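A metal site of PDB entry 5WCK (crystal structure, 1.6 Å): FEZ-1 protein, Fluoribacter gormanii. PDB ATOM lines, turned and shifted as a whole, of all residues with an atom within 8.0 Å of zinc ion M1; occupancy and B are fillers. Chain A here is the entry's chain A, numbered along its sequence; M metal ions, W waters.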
ATOM      1  N   SER A  70       6.818  -5.249  26.594  1.00  0.00           N
ATOM      2  CA  SER A  70       7.493  -4.042  26.117  1.00  0.00           C
ATOM      3  C   SER A  70       8.067  -4.246  24.716  1.00  0.00           C
ATOM      4  O   SER A  70       7.960  -3.395  23.853  1.00  0.00           O
ATOM      5  CB  SER A  70       8.601  -3.626  27.057  1.00  0.00           C
ATOM      6  OG  SER A  70       8.064  -3.162  28.290  1.00  0.00           O
ATOM      7  N   HIS A  71       8.767  -5.363  24.530  1.00  0.00           N
ATOM      8  CA  HIS A  71       9.333  -5.671  23.226  1.00  0.00           C
ATOM      9  C   HIS A  71       9.751  -7.147  23.179  1.00  0.00           C
ATOM     10  O   HIS A  71       9.878  -7.786  24.211  1.00  0.00           O
ATOM     11  CB  HIS A  71      10.491  -4.723  22.873  1.00  0.00           C
ATOM     12  CG  HIS A  71      11.733  -4.834  23.693  1.00  0.00           C
ATOM     13  ND1 HIS A  71      12.029  -3.955  24.737  1.00  0.00           N
ATOM     14  CD2 HIS A  71      12.779  -5.673  23.603  1.00  0.00           C
ATOM     15  CE1 HIS A  71      13.214  -4.265  25.226  1.00  0.00           C
ATOM     16  NE2 HIS A  71      13.708  -5.306  24.551  1.00  0.00           N
ATOM     17  N   ALA A  72       9.976  -7.637  21.954  1.00  0.00           N
ATOM     18  CA  ALA A  72      10.207  -9.073  21.694  1.00  0.00           C
ATOM     19  C   ALA A  72      11.699  -9.414  21.818  1.00  0.00           C
ATOM     20  O   ALA A  72      12.364  -9.683  20.837  1.00  0.00           O
ATOM     21  CB  ALA A  72       9.666  -9.451  20.335  1.00  0.00           C
ATOM     22  N   HIS A  73      12.204  -9.414  23.054  1.00  0.00           N
ATOM     23  CA  HIS A  73      13.464 -10.007  23.427  1.00  0.00           C
ATOM     24  C   HIS A  73      13.217 -10.980  24.595  1.00  0.00           C
ATOM     25  O   HIS A  73      12.291 -10.806  25.383  1.00  0.00           O
ATOM     26  CB  HIS A  73      14.512  -8.957  23.807  1.00  0.00           C
ATOM     27  CG  HIS A  73      15.164  -8.289  22.650  1.00  0.00           C
ATOM     28  ND1 HIS A  73      15.768  -7.019  22.763  1.00  0.00           N
ATOM     29  CD2 HIS A  73      15.346  -8.693  21.372  1.00  0.00           C
ATOM     30  CE1 HIS A  73      16.290  -6.708  21.583  1.00  0.00           C
ATOM     31  NE2 HIS A  73      16.019  -7.682  20.713  1.00  0.00           N
ATOM     32  N   PHE A  74      14.084 -11.989  24.706  1.00  0.00           N
ATOM     33  CA  PHE A  74      13.897 -13.041  25.705  1.00  0.00           C
ATOM     34  C   PHE A  74      13.756 -12.496  27.128  1.00  0.00           C
ATOM     35  O   PHE A  74      13.022 -13.097  27.929  1.00  0.00           O
ATOM     36  CB  PHE A  74      15.046 -14.067  25.643  1.00  0.00           C
ATOM     37  CG  PHE A  74      16.339 -13.554  26.207  1.00  0.00           C
ATOM     38  CD1 PHE A  74      17.214 -12.819  25.433  1.00  0.00           C
ATOM     39  CD2 PHE A  74      16.672 -13.764  27.534  1.00  0.00           C
ATOM     40  CE1 PHE A  74      18.393 -12.302  25.965  1.00  0.00           C
ATOM     41  CE2 PHE A  74      17.842 -13.257  28.072  1.00  0.00           C
ATOM     42  CZ  PHE A  74      18.703 -12.515  27.289  1.00  0.00           C
ATOM     43  N   ASP A  75      14.446 -11.398  27.459  1.00  0.00           N
ATOM     44  CA  ASP A  75      14.445 -10.905  28.835  1.00  0.00           C
ATOM     45  C   ASP A  75      13.095 -10.289  29.208  1.00  0.00           C
ATOM     46  O   ASP A  75      12.854 -10.101  30.398  1.00  0.00           O
ATOM     47  CB  ASP A  75      15.604  -9.940  29.112  1.00  0.00           C
ATOM     48  CG  ASP A  75      15.706  -8.715  28.218  1.00  0.00           C
ATOM     49  OD1 ASP A  75      15.405  -8.859  27.027  1.00  0.00           O
ATOM     50  OD2 ASP A  75      16.149  -7.648  28.706  1.00  0.00           O
ATOM     51  N   HIS A  76      12.244  -9.960  28.224  1.00  0.00           N
ATOM     52  CA  HIS A  76      10.904  -9.431  28.505  1.00  0.00           C
ATOM     53  C   HIS A  76       9.789 -10.416  28.166  1.00  0.00           C
ATOM     54  O   HIS A  76       8.686 -10.255  28.714  1.00  0.00           O
ATOM     55  CB  HIS A  76      10.709  -8.085  27.782  1.00  0.00           C
ATOM     56  CG  HIS A  76      11.825  -7.151  28.096  1.00  0.00           C
ATOM     57  ND1 HIS A  76      11.985  -6.591  29.339  1.00  0.00           N
ATOM     58  CD2 HIS A  76      12.918  -6.805  27.391  1.00  0.00           C
ATOM     59  CE1 HIS A  76      13.117  -5.911  29.365  1.00  0.00           C
ATOM     60  NE2 HIS A  76      13.692  -5.979  28.190  1.00  0.00           N
ATOM     61  N   ASP A 108      14.674 -12.881  14.521  1.00  0.00           N
ATOM     62  CA  ASP A 108      15.135 -11.574  15.023  1.00  0.00           C
ATOM     63  C   ASP A 108      16.125 -10.976  14.031  1.00  0.00           C
ATOM     64  O   ASP A 108      17.059 -11.658  13.570  1.00  0.00           O
ATOM     65  CB  ASP A 108      15.766 -11.750  16.398  1.00  0.00           C
ATOM     66  CG  ASP A 108      16.072 -10.445  17.119  1.00  0.00           C
ATOM     67  OD1 ASP A 108      17.040  -9.746  16.698  1.00  0.00           O
ATOM     68  OD2 ASP A 108      15.350 -10.156  18.076  1.00  0.00           O
ATOM     69  N   TYR A 111      19.554 -11.113  16.196  1.00  0.00           N
ATOM     70  CA  TYR A 111      19.951 -12.254  17.067  1.00  0.00           C
ATOM     71  C   TYR A 111      19.475 -13.603  16.485  1.00  0.00           C
ATOM     72  O   TYR A 111      19.543 -14.615  17.176  1.00  0.00           O
ATOM     73  CB  TYR A 111      19.414 -12.092  18.495  1.00  0.00           C
ATOM     74  CG  TYR A 111      19.964 -10.883  19.208  1.00  0.00           C
ATOM     75  CD1 TYR A 111      21.265 -10.853  19.675  1.00  0.00           C
ATOM     76  CD2 TYR A 111      19.173  -9.768  19.401  1.00  0.00           C
ATOM     77  CE1 TYR A 111      21.764  -9.739  20.340  1.00  0.00           C
ATOM     78  CE2 TYR A 111      19.670  -8.628  20.023  1.00  0.00           C
ATOM     79  CZ  TYR A 111      20.962  -8.607  20.497  1.00  0.00           C
ATOM     80  OH  TYR A 111      21.481  -7.505  21.126  1.00  0.00           O
ATOM     81  N   HIS A 149      14.971  -0.455  18.766  1.00  0.00           N
ATOM     82  CA  HIS A 149      15.496  -1.474  19.660  1.00  0.00           C
ATOM     83  C   HIS A 149      15.001  -2.863  19.233  1.00  0.00           C
ATOM     84  O   HIS A 149      15.766  -3.832  19.238  1.00  0.00           O
ATOM     85  CB  HIS A 149      15.189  -1.145  21.129  1.00  0.00           C
ATOM     86  CG  HIS A 149      15.748  -2.148  22.062  1.00  0.00           C
ATOM     87  ND1 HIS A 149      17.069  -2.121  22.491  1.00  0.00           N
ATOM     88  CD2 HIS A 149      15.181  -3.252  22.600  1.00  0.00           C
ATOM     89  CE1 HIS A 149      17.278  -3.176  23.276  1.00  0.00           C
ATOM     90  NE2 HIS A 149      16.137  -3.879  23.362  1.00  0.00           N
ATOM     91  N   THR A 150      13.699  -2.955  18.946  1.00  0.00           N
ATOM     92  CA  THR A 150      13.122  -4.023  18.154  1.00  0.00           C
ATOM     93  C   THR A 150      12.203  -3.383  17.129  1.00  0.00           C
ATOM     94  O   THR A 150      11.890  -2.192  17.197  1.00  0.00           O
ATOM     95  CB  THR A 150      12.331  -5.054  18.982  1.00  0.00           C
ATOM     96  OG1 THR A 150      11.136  -4.437  19.450  1.00  0.00           O
ATOM     97  CG2 THR A 150      13.130  -5.650  20.118  1.00  0.00           C
ATOM     98  N   CYS A 153       8.958  -2.502  19.123  1.00  0.00           N
ATOM     99  CA  CYS A 153       9.059  -2.076  20.504  1.00  0.00           C
ATOM    100  C   CYS A 153       7.902  -1.134  20.835  1.00  0.00           C
ATOM    101  O   CYS A 153       7.600  -0.205  20.039  1.00  0.00           O
ATOM    102  CB  CYS A 153      10.386  -1.367  20.724  1.00  0.00           C
ATOM    103  SG  CYS A 153      10.575  -0.860  22.459  1.00  0.00           S
ATOM    104  N   GLY A 173       9.506   1.359  26.352  1.00  0.00           N
ATOM    105  CA  GLY A 173       9.803  -0.021  25.915  1.00  0.00           C
ATOM    106  C   GLY A 173      11.279  -0.387  25.886  1.00  0.00           C
ATOM    107  O   GLY A 173      11.603  -1.523  26.230  1.00  0.00           O
ATOM    108  N   SER A 174      12.048   0.579  25.382  1.00  0.00           N
ATOM    109  CA  SER A 174      13.531   0.717  25.213  1.00  0.00           C
ATOM    110  C   SER A 174      13.833   1.476  23.920  1.00  0.00           C
ATOM    111  O   SER A 174      13.287   1.114  22.926  1.00  0.00           O
ATOM    112  CB  SER A 174      14.358  -0.546  25.132  1.00  0.00           C
ATOM    113  OG  SER A 174      15.700  -0.256  24.849  1.00  0.00           O
ATOM    114  N   GLY A 176      17.338   1.855  23.550  1.00  0.00           N
ATOM    115  CA  GLY A 176      18.746   1.556  23.629  1.00  0.00           C
ATOM    116  C   GLY A 176      19.271   0.935  22.348  1.00  0.00           C
ATOM    117  O   GLY A 176      18.554   0.166  21.698  1.00  0.00           O
ATOM    118  N   ASN A 178      21.741  -1.746  21.236  1.00  0.00           N
ATOM    119  CA  ASN A 178      22.506  -2.842  21.826  1.00  0.00           C
ATOM    120  C   ASN A 178      23.890  -2.922  21.191  1.00  0.00           C
ATOM    121  O   ASN A 178      24.074  -2.590  20.033  1.00  0.00           O
ATOM    122  CB  ASN A 178      21.805  -4.181  21.681  1.00  0.00           C
ATOM    123  CG  ASN A 178      20.672  -4.348  22.676  1.00  0.00           C
ATOM    124  OD1 ASN A 178      20.442  -3.482  23.535  1.00  0.00           O
ATOM    125  ND2 ASN A 178      19.973  -5.460  22.600  1.00  0.00           N
ATOM    126  N   TYR A 181      24.757  -3.601  17.286  1.00  0.00           N
ATOM    127  CA  TYR A 181      23.689  -3.240  16.337  1.00  0.00           C
ATOM    128  C   TYR A 181      24.308  -2.401  15.214  1.00  0.00           C
ATOM    129  O   TYR A 181      25.097  -1.577  15.540  1.00  0.00           O
ATOM    130  CB  TYR A 181      22.649  -2.369  17.038  1.00  0.00           C
ATOM    131  CG  TYR A 181      21.446  -3.077  17.616  1.00  0.00           C
ATOM    132  CD1 TYR A 181      21.467  -4.436  17.863  1.00  0.00           C
ATOM    133  CD2 TYR A 181      20.298  -2.380  17.916  1.00  0.00           C
ATOM    134  CE1 TYR A 181      20.368  -5.080  18.394  1.00  0.00           C
ATOM    135  CE2 TYR A 181      19.189  -3.006  18.443  1.00  0.00           C
ATOM    136  CZ  TYR A 181      19.216  -4.368  18.678  1.00  0.00           C
ATOM    137  OH  TYR A 181      18.133  -5.008  19.191  1.00  0.00           O
ATOM    138  N   SER A 214      11.037  -0.890  30.840  1.00  0.00           N
ATOM    139  CA  SER A 214      11.180  -2.356  30.776  1.00  0.00           C
ATOM    140  C   SER A 214      12.273  -2.873  31.732  1.00  0.00           C
ATOM    141  O   SER A 214      12.251  -4.058  32.082  1.00  0.00           O
ATOM    142  CB  SER A 214      11.408  -2.771  29.375  1.00  0.00           C
ATOM    143  OG  SER A 214      12.528  -2.106  28.807  1.00  0.00           O
ATOM    144  N   HIS A 215      13.212  -2.014  32.131  1.00  0.00           N
ATOM    145  CA  HIS A 215      14.234  -2.341  33.092  1.00  0.00           C
ATOM    146  C   HIS A 215      14.207  -1.330  34.255  1.00  0.00           C
ATOM    147  O   HIS A 215      14.102  -0.116  34.035  1.00  0.00           O
ATOM    148  CB  HIS A 215      15.646  -2.362  32.471  1.00  0.00           C
ATOM    149  CG  HIS A 215      15.885  -3.468  31.511  1.00  0.00           C
ATOM    150  ND1 HIS A 215      16.514  -4.634  31.903  1.00  0.00           N
ATOM    151  CD2 HIS A 215      15.571  -3.622  30.207  1.00  0.00           C
ATOM    152  CE1 HIS A 215      16.609  -5.436  30.862  1.00  0.00           C
ATOM    153  NE2 HIS A 215      16.045  -4.850  29.811  1.00  0.00           N
ATOM    154  N   MET A 218      16.372   1.879  34.277  1.00  0.00           N
ATOM    155  CA  MET A 218      16.019   3.016  33.416  1.00  0.00           C
ATOM    156  C   MET A 218      15.457   4.150  34.267  1.00  0.00           C
ATOM    157  O   MET A 218      15.672   5.331  33.936  1.00  0.00           O
ATOM    158  CB  MET A 218      14.956   2.620  32.377  1.00  0.00           C
ATOM    159  CG  MET A 218      15.483   1.635  31.413  1.00  0.00           C
ATOM    160  SD  MET A 218      14.109   1.032  30.384  1.00  0.00           S
ATOM    161  CE  MET A 218      15.000   0.275  29.027  1.00  0.00           C
HETATM  162 ZN    ZN M   1      15.752  -5.682  24.323  1.00  0.00          ZN
HETATM  163 ZN    ZN M   2      15.826  -5.756  27.982  1.00  0.00          ZN
HETATM  164  O   HOH W   1      16.304  -6.318  26.112  1.00  0.00           O
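A ring nitrogen (ND1) of His 149 is in hydrogen-bond range of the side-chain hydroxyl of Ser 174. The backbone carbonyl oxygen of His 149 is in hydrogen-bond range of the side-chain hydroxyl of Tyr 181. The backbone carbonyl oxygen of Gly 176 lies within hydrogen-bond range of a ring nitrogen (ND1) of His 149, 2.8 Å away. The backbone carbonyl oxygen of Gly 173 is in hydrogen-bond range of a ring nitrogen (ND1) of His 71.
Within 4 Å of zinc ion M1: His 71, His 73 and His 149.
Water W1 is bound to zinc ion M1 (2.0 Å). Zinc ion M1 is bound by ND1 of His 73 (2.1 Å). A ring nitrogen (NE2) of His 149 binds zinc ion M1 (2.1 Å). Zinc ion M1 is bound by a ring nitrogen (NE2) of His 71. Zinc ion M1 has four donor atoms within binding distance.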
